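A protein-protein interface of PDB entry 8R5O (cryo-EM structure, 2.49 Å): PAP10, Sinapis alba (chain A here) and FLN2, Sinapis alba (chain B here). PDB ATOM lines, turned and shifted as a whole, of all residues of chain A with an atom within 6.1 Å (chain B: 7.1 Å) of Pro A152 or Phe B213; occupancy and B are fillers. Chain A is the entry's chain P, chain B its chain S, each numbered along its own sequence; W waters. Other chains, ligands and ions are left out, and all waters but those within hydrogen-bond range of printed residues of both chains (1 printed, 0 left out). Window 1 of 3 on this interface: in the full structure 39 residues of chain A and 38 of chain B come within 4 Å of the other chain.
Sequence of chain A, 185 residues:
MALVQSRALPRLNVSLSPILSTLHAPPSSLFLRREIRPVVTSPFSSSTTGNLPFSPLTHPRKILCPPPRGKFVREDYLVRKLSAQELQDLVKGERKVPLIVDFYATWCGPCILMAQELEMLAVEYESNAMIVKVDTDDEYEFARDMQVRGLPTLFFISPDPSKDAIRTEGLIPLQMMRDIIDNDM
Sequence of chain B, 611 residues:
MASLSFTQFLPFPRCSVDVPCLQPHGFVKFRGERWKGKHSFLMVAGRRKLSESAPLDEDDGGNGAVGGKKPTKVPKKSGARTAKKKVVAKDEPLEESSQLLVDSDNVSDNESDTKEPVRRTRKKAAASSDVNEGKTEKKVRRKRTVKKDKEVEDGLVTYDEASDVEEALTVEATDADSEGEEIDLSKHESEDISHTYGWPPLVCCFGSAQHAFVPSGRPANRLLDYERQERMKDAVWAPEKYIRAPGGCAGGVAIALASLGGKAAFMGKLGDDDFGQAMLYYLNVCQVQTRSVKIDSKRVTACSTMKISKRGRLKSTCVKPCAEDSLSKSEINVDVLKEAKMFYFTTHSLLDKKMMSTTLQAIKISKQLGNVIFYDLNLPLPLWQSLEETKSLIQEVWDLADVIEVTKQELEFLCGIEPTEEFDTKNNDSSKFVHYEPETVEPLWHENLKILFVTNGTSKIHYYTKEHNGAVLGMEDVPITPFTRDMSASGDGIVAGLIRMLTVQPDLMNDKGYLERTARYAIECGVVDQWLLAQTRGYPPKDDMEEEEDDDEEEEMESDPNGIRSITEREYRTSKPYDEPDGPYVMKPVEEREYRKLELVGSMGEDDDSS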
ATOM      1  N   ASP A 102     -20.508 -27.898   3.421  1.00  0.00           N
ATOM      2  CA  ASP A 102     -19.140 -27.651   2.973  1.00  0.00           C
ATOM      3  C   ASP A 102     -18.464 -26.708   3.964  1.00  0.00           C
ATOM      4  O   ASP A 102     -18.615 -25.487   3.875  1.00  0.00           O
ATOM      5  CB  ASP A 102     -19.140 -27.079   1.559  1.00  0.00           C
ATOM      6  CG  ASP A 102     -17.792 -26.517   1.151  1.00  0.00           C
ATOM      7  OD1 ASP A 102     -16.806 -27.283   1.119  1.00  0.00           O
ATOM      8  OD2 ASP A 102     -17.720 -25.306   0.854  1.00  0.00           O
ATOM      9  N   PHE A 103     -17.726 -27.275   4.912  1.00  0.00           N
ATOM     10  CA  PHE A 103     -16.914 -26.459   5.806  1.00  0.00           C
ATOM     11  C   PHE A 103     -15.735 -25.880   5.035  1.00  0.00           C
ATOM     12  O   PHE A 103     -15.008 -26.609   4.354  1.00  0.00           O
ATOM     13  CB  PHE A 103     -16.422 -27.288   6.990  1.00  0.00           C
ATOM     14  CG  PHE A 103     -17.510 -27.699   7.938  1.00  0.00           C
ATOM     15  CD1 PHE A 103     -18.209 -28.876   7.740  1.00  0.00           C
ATOM     16  CD2 PHE A 103     -17.829 -26.911   9.029  1.00  0.00           C
ATOM     17  CE1 PHE A 103     -19.207 -29.255   8.608  1.00  0.00           C
ATOM     18  CE2 PHE A 103     -18.827 -27.286   9.901  1.00  0.00           C
ATOM     19  CZ  PHE A 103     -19.516 -28.460   9.692  1.00  0.00           C
ATOM     20  N   TYR A 104     -15.538 -24.569   5.144  1.00  0.00           N
ATOM     21  CA  TYR A 104     -14.513 -23.900   4.362  1.00  0.00           C
ATOM     22  C   TYR A 104     -13.987 -22.693   5.128  1.00  0.00           C
ATOM     23  O   TYR A 104     -14.534 -22.294   6.158  1.00  0.00           O
ATOM     24  CB  TYR A 104     -15.048 -23.464   2.995  1.00  0.00           C
ATOM     25  CG  TYR A 104     -15.919 -22.230   3.064  1.00  0.00           C
ATOM     26  CD1 TYR A 104     -17.240 -22.316   3.477  1.00  0.00           C
ATOM     27  CD2 TYR A 104     -15.418 -20.981   2.723  1.00  0.00           C
ATOM     28  CE1 TYR A 104     -18.035 -21.195   3.548  1.00  0.00           C
ATOM     29  CE2 TYR A 104     -16.209 -19.851   2.794  1.00  0.00           C
ATOM     30  CZ  TYR A 104     -17.519 -19.966   3.205  1.00  0.00           C
ATOM     31  OH  TYR A 104     -18.322 -18.852   3.280  1.00  0.00           O
ATOM     32  N   CYS A 108      -8.039 -20.754   2.483  1.00  0.00           N
ATOM     33  CA  CYS A 108      -7.614 -22.074   2.031  1.00  0.00           C
ATOM     34  C   CYS A 108      -7.775 -22.178   0.519  1.00  0.00           C
ATOM     35  O   CYS A 108      -8.888 -22.062  -0.005  1.00  0.00           O
ATOM     36  CB  CYS A 108      -8.412 -23.172   2.735  1.00  0.00           C
ATOM     37  SG  CYS A 108      -7.876 -24.854   2.356  1.00  0.00           S
ATOM     38  N   PRO A 110      -7.278 -24.930  -1.563  1.00  0.00           N
ATOM     39  CA  PRO A 110      -8.085 -26.080  -2.008  1.00  0.00           C
ATOM     40  C   PRO A 110      -9.577 -25.914  -1.780  1.00  0.00           C
ATOM     41  O   PRO A 110     -10.372 -26.516  -2.510  1.00  0.00           O
ATOM     42  CB  PRO A 110      -7.513 -27.244  -1.190  1.00  0.00           C
ATOM     43  CG  PRO A 110      -6.112 -26.845  -0.920  1.00  0.00           C
ATOM     44  CD  PRO A 110      -6.139 -25.357  -0.730  1.00  0.00           C
ATOM     45  N   CYS A 111      -9.989 -25.128  -0.782  1.00  0.00           N
ATOM     46  CA  CYS A 111     -11.415 -24.880  -0.585  1.00  0.00           C
ATOM     47  C   CYS A 111     -12.016 -24.121  -1.760  1.00  0.00           C
ATOM     48  O   CYS A 111     -13.203 -24.281  -2.060  1.00  0.00           O
ATOM     49  CB  CYS A 111     -11.646 -24.112   0.716  1.00  0.00           C
ATOM     50  SG  CYS A 111     -11.425 -25.094   2.213  1.00  0.00           S
ATOM     51  N   MET A 114     -12.593 -26.728  -4.316  1.00  0.00           N
ATOM     52  CA  MET A 114     -13.767 -27.496  -3.914  1.00  0.00           C
ATOM     53  C   MET A 114     -15.056 -26.754  -4.243  1.00  0.00           C
ATOM     54  O   MET A 114     -16.069 -27.383  -4.568  1.00  0.00           O
ATOM     55  CB  MET A 114     -13.691 -27.813  -2.420  1.00  0.00           C
ATOM     56  CG  MET A 114     -14.927 -28.481  -1.838  1.00  0.00           C
ATOM     57  SD  MET A 114     -15.235 -30.136  -2.485  1.00  0.00           S
ATOM     58  CE  MET A 114     -13.895 -31.060  -1.735  1.00  0.00           C
ATOM     59  N   ARG A 149     -11.525 -31.695  11.261  1.00  0.00           N
ATOM     60  CA  ARG A 149     -10.108 -31.731  11.593  1.00  0.00           C
ATOM     61  C   ARG A 149      -9.244 -30.998  10.581  1.00  0.00           C
ATOM     62  O   ARG A 149      -8.015 -31.040  10.687  1.00  0.00           O
ATOM     63  CB  ARG A 149      -9.642 -33.183  11.728  1.00  0.00           C
ATOM     64  CG  ARG A 149     -10.559 -34.018  12.609  1.00  0.00           C
ATOM     65  CD  ARG A 149      -9.993 -35.392  12.877  1.00  0.00           C
ATOM     66  NE  ARG A 149      -9.840 -36.172  11.659  1.00  0.00           N
ATOM     67  CZ  ARG A 149      -9.440 -37.434  11.630  1.00  0.00           C
ATOM     68  NH1 ARG A 149      -9.157 -38.093  12.741  1.00  0.00           N
ATOM     69  NH2 ARG A 149      -9.323 -38.051  10.458  1.00  0.00           N
ATOM     70  N   GLY A 150      -9.851 -30.330   9.610  1.00  0.00           N
ATOM     71  CA  GLY A 150      -9.097 -29.629   8.593  1.00  0.00           C
ATOM     72  C   GLY A 150     -10.009 -29.244   7.447  1.00  0.00           C
ATOM     73  O   GLY A 150     -11.222 -29.454   7.500  1.00  0.00           O
ATOM     74  N   LEU A 151      -9.399 -28.683   6.405  1.00  0.00           N
ATOM     75  CA  LEU A 151     -10.151 -28.173   5.275  1.00  0.00           C
ATOM     76  C   LEU A 151      -9.523 -28.630   3.965  1.00  0.00           C
ATOM     77  O   LEU A 151      -8.292 -28.750   3.877  1.00  0.00           O
ATOM     78  CB  LEU A 151     -10.219 -26.640   5.314  1.00  0.00           C
ATOM     79  CG  LEU A 151     -10.892 -26.062   6.563  1.00  0.00           C
ATOM     80  CD1 LEU A 151     -10.727 -24.560   6.611  1.00  0.00           C
ATOM     81  CD2 LEU A 151     -12.364 -26.447   6.614  1.00  0.00           C
ATOM     82  N   PRO A 152     -10.339 -28.898   2.934  1.00  0.00           N
ATOM     83  CA  PRO A 152     -11.808 -28.862   2.918  1.00  0.00           C
ATOM     84  C   PRO A 152     -12.437 -30.085   3.584  1.00  0.00           C
ATOM     85  O   PRO A 152     -11.816 -31.139   3.690  1.00  0.00           O
ATOM     86  CB  PRO A 152     -12.127 -28.794   1.419  1.00  0.00           C
ATOM     87  CG  PRO A 152     -11.010 -29.560   0.779  1.00  0.00           C
ATOM     88  CD  PRO A 152      -9.788 -29.255   1.612  1.00  0.00           C
ATOM     89  N   THR A 153     -13.679 -29.955   4.051  1.00  0.00           N
ATOM     90  CA  THR A 153     -14.400 -31.032   4.713  1.00  0.00           C
ATOM     91  C   THR A 153     -15.863 -30.971   4.303  1.00  0.00           C
ATOM     92  O   THR A 153     -16.491 -29.915   4.400  1.00  0.00           O
ATOM     93  CB  THR A 153     -14.277 -30.930   6.241  1.00  0.00           C
ATOM     94  OG1 THR A 153     -13.014 -31.455   6.660  1.00  0.00           O
ATOM     95  CG2 THR A 153     -15.400 -31.698   6.933  1.00  0.00           C
ATOM     96  N   LEU A 154     -16.399 -32.099   3.846  1.00  0.00           N
ATOM     97  CA  LEU A 154     -17.788 -32.191   3.422  1.00  0.00           C
ATOM     98  C   LEU A 154     -18.547 -33.137   4.340  1.00  0.00           C
ATOM     99  O   LEU A 154     -18.017 -34.169   4.761  1.00  0.00           O
ATOM    100  CB  LEU A 154     -17.902 -32.679   1.976  1.00  0.00           C
ATOM    101  CG  LEU A 154     -17.091 -31.939   0.912  1.00  0.00           C
ATOM    102  CD1 LEU A 154     -17.369 -32.527  -0.457  1.00  0.00           C
ATOM    103  CD2 LEU A 154     -17.397 -30.455   0.934  1.00  0.00           C
ATOM    104  N   THR A 168     -16.143 -36.417   4.597  1.00  0.00           N
ATOM    105  CA  THR A 168     -15.034 -36.573   3.668  1.00  0.00           C
ATOM    106  C   THR A 168     -14.021 -35.459   3.895  1.00  0.00           C
ATOM    107  O   THR A 168     -14.392 -34.314   4.167  1.00  0.00           O
ATOM    108  CB  THR A 168     -15.506 -36.562   2.213  1.00  0.00           C
ATOM    109  OG1 THR A 168     -15.930 -35.242   1.850  1.00  0.00           O
ATOM    110  CG2 THR A 168     -16.660 -37.534   2.018  1.00  0.00           C
ATOM    111  N   GLU A 169     -12.742 -35.804   3.785  1.00  0.00           N
ATOM    112  CA  GLU A 169     -11.649 -34.873   4.012  1.00  0.00           C
ATOM    113  C   GLU A 169     -10.768 -34.797   2.776  1.00  0.00           C
ATOM    114  O   GLU A 169     -10.434 -35.821   2.174  1.00  0.00           O
ATOM    115  CB  GLU A 169     -10.816 -35.289   5.224  1.00  0.00           C
ATOM    116  CG  GLU A 169     -11.494 -35.030   6.553  1.00  0.00           C
ATOM    117  CD  GLU A 169     -10.796 -35.724   7.701  1.00  0.00           C
ATOM    118  OE1 GLU A 169     -10.198 -36.794   7.467  1.00  0.00           O
ATOM    119  OE2 GLU A 169     -10.839 -35.199   8.832  1.00  0.00           O
ATOM    120  N   GLY A 170     -10.393 -33.577   2.403  1.00  0.00           N
ATOM    121  CA  GLY A 170      -9.557 -33.360   1.244  1.00  0.00           C
ATOM    122  C   GLY A 170     -10.356 -33.095  -0.014  1.00  0.00           C
ATOM    123  O   GLY A 170     -11.588 -33.065  -0.030  1.00  0.00           O
ATOM    124  N   LEU A 171      -9.619 -32.899  -1.103  1.00  0.00           N
ATOM    125  CA  LEU A 171     -10.212 -32.606  -2.405  1.00  0.00           C
ATOM    126  C   LEU A 171     -10.521 -33.933  -3.089  1.00  0.00           C
ATOM    127  O   LEU A 171      -9.639 -34.564  -3.677  1.00  0.00           O
ATOM    128  CB  LEU A 171      -9.269 -31.741  -3.234  1.00  0.00           C
ATOM    129  CG  LEU A 171      -9.838 -30.929  -4.394  1.00  0.00           C
ATOM    130  CD1 LEU A 171     -11.085 -30.172  -3.970  1.00  0.00           C
ATOM    131  CD2 LEU A 171      -8.779 -29.964  -4.893  1.00  0.00           C
ATOM    132  N   GLN B 210      -3.311 -37.777   2.323  1.00  0.00           N
ATOM    133  CA  GLN B 210      -4.486 -37.036   1.895  1.00  0.00           C
ATOM    134  C   GLN B 210      -4.166 -36.209   0.655  1.00  0.00           C
ATOM    135  O   GLN B 210      -3.010 -36.057   0.257  1.00  0.00           O
ATOM    136  CB  GLN B 210      -4.995 -36.145   3.029  1.00  0.00           C
ATOM    137  CG  GLN B 210      -5.607 -36.921   4.180  1.00  0.00           C
ATOM    138  CD  GLN B 210      -5.315 -36.297   5.525  1.00  0.00           C
ATOM    139  OE1 GLN B 210      -4.392 -35.497   5.666  1.00  0.00           O
ATOM    140  NE2 GLN B 210      -6.103 -36.661   6.527  1.00  0.00           N
ATOM    141  N   HIS B 211      -5.215 -35.670   0.043  1.00  0.00           N
ATOM    142  CA  HIS B 211      -5.093 -34.888  -1.184  1.00  0.00           C
ATOM    143  C   HIS B 211      -5.543 -33.463  -0.904  1.00  0.00           C
ATOM    144  O   HIS B 211      -6.729 -33.221  -0.660  1.00  0.00           O
ATOM    145  CB  HIS B 211      -5.909 -35.512  -2.314  1.00  0.00           C
ATOM    146  CG  HIS B 211      -5.779 -34.792  -3.619  1.00  0.00           C
ATOM    147  ND1 HIS B 211      -6.869 -34.390  -4.360  1.00  0.00           N
ATOM    148  CD2 HIS B 211      -4.686 -34.395  -4.312  1.00  0.00           C
ATOM    149  CE1 HIS B 211      -6.453 -33.781  -5.455  1.00  0.00           C
ATOM    150  NE2 HIS B 211      -5.132 -33.770  -5.450  1.00  0.00           N
ATOM    151  N   ALA B 212      -4.594 -32.527  -0.947  1.00  0.00           N
ATOM    152  CA  ALA B 212      -4.853 -31.102  -0.744  1.00  0.00           C
ATOM    153  C   ALA B 212      -5.665 -30.865   0.530  1.00  0.00           C
ATOM    154  O   ALA B 212      -6.756 -30.293   0.514  1.00  0.00           O
ATOM    155  CB  ALA B 212      -5.546 -30.498  -1.966  1.00  0.00           C
ATOM    156  N   PHE B 213      -5.111 -31.329   1.644  1.00  0.00           N
ATOM    157  CA  PHE B 213      -5.747 -31.225   2.949  1.00  0.00           C
ATOM    158  C   PHE B 213      -4.880 -30.363   3.855  1.00  0.00           C
ATOM    159  O   PHE B 213      -3.667 -30.569   3.936  1.00  0.00           O
ATOM    160  CB  PHE B 213      -5.959 -32.611   3.561  1.00  0.00           C
ATOM    161  CG  PHE B 213      -6.893 -32.621   4.731  1.00  0.00           C
ATOM    162  CD1 PHE B 213      -8.233 -32.321   4.565  1.00  0.00           C
ATOM    163  CD2 PHE B 213      -6.439 -32.948   5.996  1.00  0.00           C
ATOM    164  CE1 PHE B 213      -9.098 -32.331   5.635  1.00  0.00           C
ATOM    165  CE2 PHE B 213      -7.300 -32.965   7.073  1.00  0.00           C
ATOM    166  CZ  PHE B 213      -8.631 -32.660   6.892  1.00  0.00           C
ATOM    167  N   VAL B 214      -5.506 -29.405   4.531  1.00  0.00           N
ATOM    168  CA  VAL B 214      -4.812 -28.418   5.345  1.00  0.00           C
ATOM    169  C   VAL B 214      -5.241 -28.610   6.792  1.00  0.00           C
ATOM    170  O   VAL B 214      -6.440 -28.613   7.075  1.00  0.00           O
ATOM    171  CB  VAL B 214      -5.103 -26.976   4.892  1.00  0.00           C
ATOM    172  CG1 VAL B 214      -4.468 -25.988   5.848  1.00  0.00           C
ATOM    173  CG2 VAL B 214      -4.594 -26.756   3.479  1.00  0.00           C
ATOM    174  N   PRO B 215      -4.307 -28.772   7.735  1.00  0.00           N
ATOM    175  CA  PRO B 215      -4.720 -28.928   9.139  1.00  0.00           C
ATOM    176  C   PRO B 215      -5.270 -27.654   9.752  1.00  0.00           C
ATOM    177  O   PRO B 215      -6.303 -27.701  10.432  1.00  0.00           O
ATOM    178  CB  PRO B 215      -3.426 -29.378   9.837  1.00  0.00           C
ATOM    179  CG  PRO B 215      -2.514 -29.824   8.735  1.00  0.00           C
ATOM    180  CD  PRO B 215      -2.864 -28.983   7.557  1.00  0.00           C
ATOM    181  N   SER B 216      -4.614 -26.515   9.542  1.00  0.00           N
ATOM    182  CA  SER B 216      -5.015 -25.276  10.195  1.00  0.00           C
ATOM    183  C   SER B 216      -4.389 -24.100   9.459  1.00  0.00           C
ATOM    184  O   SER B 216      -3.571 -24.269   8.555  1.00  0.00           O
ATOM    185  CB  SER B 216      -4.611 -25.269  11.671  1.00  0.00           C
ATOM    186  OG  SER B 216      -3.204 -25.364  11.812  1.00  0.00           O
ATOM    187  N   GLY B 247       1.584 -26.747   7.011  1.00  0.00           N
ATOM    188  CA  GLY B 247       2.018 -27.740   6.049  1.00  0.00           C
ATOM    189  C   GLY B 247       0.852 -28.632   5.662  1.00  0.00           C
ATOM    190  O   GLY B 247      -0.307 -28.239   5.767  1.00  0.00           O
ATOM    191  N   GLY B 248       1.192 -29.835   5.210  1.00  0.00           N
ATOM    192  CA  GLY B 248       0.178 -30.782   4.794  1.00  0.00           C
ATOM    193  C   GLY B 248       0.183 -32.061   5.603  1.00  0.00           C
ATOM    194  O   GLY B 248       0.298 -32.028   6.831  1.00  0.00           O
ATOM    195  N   CYS B 249       0.060 -33.195   4.920  1.00  0.00           N
ATOM    196  CA  CYS B 249       0.042 -34.503   5.549  1.00  0.00           C
ATOM    197  C   CYS B 249       1.411 -35.167   5.422  1.00  0.00           C
ATOM    198  O   CYS B 249       2.333 -34.642   4.796  1.00  0.00           O
ATOM    199  CB  CYS B 249      -1.047 -35.376   4.926  1.00  0.00           C
ATOM    200  SG  CYS B 249      -0.879 -35.606   3.142  1.00  0.00           S
ATOM    201  N   HIS B 348      -1.470 -35.185  13.428  1.00  0.00           N
ATOM    202  CA  HIS B 348      -2.711 -35.722  12.877  1.00  0.00           C
ATOM    203  C   HIS B 348      -2.889 -37.197  13.216  1.00  0.00           C
ATOM    204  O   HIS B 348      -4.023 -37.674  13.329  1.00  0.00           O
ATOM    205  CB  HIS B 348      -2.748 -35.521  11.365  1.00  0.00           C
ATOM    206  CG  HIS B 348      -3.955 -36.116  10.704  1.00  0.00           C
ATOM    207  ND1 HIS B 348      -5.152 -35.443  10.596  1.00  0.00           N
ATOM    208  CD2 HIS B 348      -4.150 -37.323  10.125  1.00  0.00           C
ATOM    209  CE1 HIS B 348      -6.031 -36.209   9.974  1.00  0.00           C
ATOM    210  NE2 HIS B 348      -5.447 -37.355   9.679  1.00  0.00           N
ATOM    211  N   ASP B 486      -2.625 -20.597   0.947  1.00  0.00           N
ATOM    212  CA  ASP B 486      -2.335 -21.020   2.311  1.00  0.00           C
ATOM    213  C   ASP B 486      -0.868 -21.366   2.535  1.00  0.00           C
ATOM    214  O   ASP B 486      -0.478 -21.603   3.684  1.00  0.00           O
ATOM    215  CB  ASP B 486      -3.207 -22.217   2.695  1.00  0.00           C
ATOM    216  CG  ASP B 486      -3.127 -23.341   1.688  1.00  0.00           C
ATOM    217  OD1 ASP B 486      -3.392 -23.093   0.492  1.00  0.00           O
ATOM    218  OD2 ASP B 486      -2.789 -24.472   2.087  1.00  0.00           O
ATOM    219  N   SER B 488       0.871 -23.966   2.040  1.00  0.00           N
ATOM    220  CA  SER B 488       1.172 -25.283   2.588  1.00  0.00           C
ATOM    221  C   SER B 488       2.263 -25.999   1.806  1.00  0.00           C
ATOM    222  O   SER B 488       2.930 -26.879   2.361  1.00  0.00           O
ATOM    223  CB  SER B 488      -0.091 -26.144   2.630  1.00  0.00           C
ATOM    224  OG  SER B 488      -0.634 -26.311   1.335  1.00  0.00           O
ATOM    225  N   ASP B 492       5.718 -28.048   3.580  1.00  0.00           N
ATOM    226  CA  ASP B 492       6.212 -29.374   3.223  1.00  0.00           C
ATOM    227  C   ASP B 492       7.614 -29.291   2.630  1.00  0.00           C
ATOM    228  O   ASP B 492       8.480 -30.114   2.946  1.00  0.00           O
ATOM    229  CB  ASP B 492       5.249 -30.045   2.247  1.00  0.00           C
ATOM    230  CG  ASP B 492       3.823 -30.078   2.766  1.00  0.00           C
ATOM    231  OD1 ASP B 492       3.632 -30.299   3.980  1.00  0.00           O
ATOM    232  OD2 ASP B 492       2.890 -29.876   1.959  1.00  0.00           O
ATOM    233  N   ARG B 537      -1.154 -25.069 -10.600  1.00  0.00           N
ATOM    234  CA  ARG B 537      -2.573 -24.865 -10.321  1.00  0.00           C
ATOM    235  C   ARG B 537      -3.151 -23.678 -11.083  1.00  0.00           C
ATOM    236  O   ARG B 537      -4.301 -23.732 -11.532  1.00  0.00           O
ATOM    237  CB  ARG B 537      -2.794 -24.691  -8.820  1.00  0.00           C
ATOM    238  CG  ARG B 537      -2.685 -25.985  -8.046  1.00  0.00           C
ATOM    239  CD  ARG B 537      -3.057 -25.799  -6.593  1.00  0.00           C
ATOM    240  NE  ARG B 537      -3.016 -27.062  -5.872  1.00  0.00           N
ATOM    241  CZ  ARG B 537      -3.120 -27.179  -4.556  1.00  0.00           C
ATOM    242  NH1 ARG B 537      -3.301 -26.124  -3.779  1.00  0.00           N
ATOM    243  NH2 ARG B 537      -3.032 -28.385  -4.005  1.00  0.00           N
HETATM  244  O   HOH W   1      -8.102 -36.840   0.635  1.00  0.00           O
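Water W1 bridges O of Glu A169 and N of His B211.
CG2 of Val B214 touches SG of Cys A108, 3.96 Å away. Pro A110 touches Asp B486. O of Arg A149 touches O of Pro B215 (3.8 Å). His B348 touches Arg A149 (CE1 to NH2, 3.8 Å). Gly A150 touches Phe B213. O of Val B214 touches CA of Gly A150, 3.2 Å away. Pro B215 touches Gly A150 (O to CA, 3.9 Å). CD of Pro A152 touches O of Ala B212, 3.4 Å away. O of Pro A152 touches CE1 of Phe B213, at 3.5 Å. His B211 touches Gly A170 (O to CA, 3.4 Å).
SG of Cys A108 lies within hydrogen-bond range of SG of Cys A111. O of Pro A152 is in hydrogen-bond range of N of Gly A170, at 3.1 Å. The side-chain carboxylate (OD2) of Asp B486 sits at hydrogen-bond distance from the side-chain hydroxyl (OG) of Ser B488 (2.9 Å). The guanidinium group of Arg A149 is in salt-bridge range of the side-chain carboxylate of Glu A169 (3.2 Å). The side-chain amide nitrogen (NE2) of Gln B210 sits at hydrogen-bond distance from a ring nitrogen (NE2) of His B348, 3.3 Å away. OG1 of Thr A153 sits at hydrogen-bond distance from O of Gly A150 (2.8 Å).
Hydrophobic or aromatic side chains of chain B within 4 Å of the printed part of chain A: His B211, Ala B212, Phe B213, Val B214 and His B348. Of the 17 printed residues of chain A, 9 touch a printed residue of chain B. Among the printed residues, 16 pairs touch across the chains. Among the printed residues, no Asp or Glu carboxylate lies within 4 Å of a Lys or Arg side-chain nitrogen of the other chain.
The backbone carbonyl oxygen of Leu A171 is in hydrogen-bond range of a ring nitrogen (ND1) of His B211 (2.9 Å). The backbone NH (N) of Val B214 is in hydrogen-bond range of the backbone carbonyl oxygen (O) of Leu A151, at 2.9 Å.
Of chain A, only Gly A150, Leu A151, Pro A152, Glu A169 and Gly A170 come within 4 Å of Phe B213. Of the printed residues of chain B, Leu A151 touches Phe B213 and Val B214. Printed residues of chain B within 4 Å of Cys A108: Val B214 (3.96 Å). Leu A154 touches none of the printed residues of chain B. Phe A103 touches none of the printed residues of chain B. The nearest residue of chain B that does not touch Pro A152 is Val B214 (5.1 Å).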
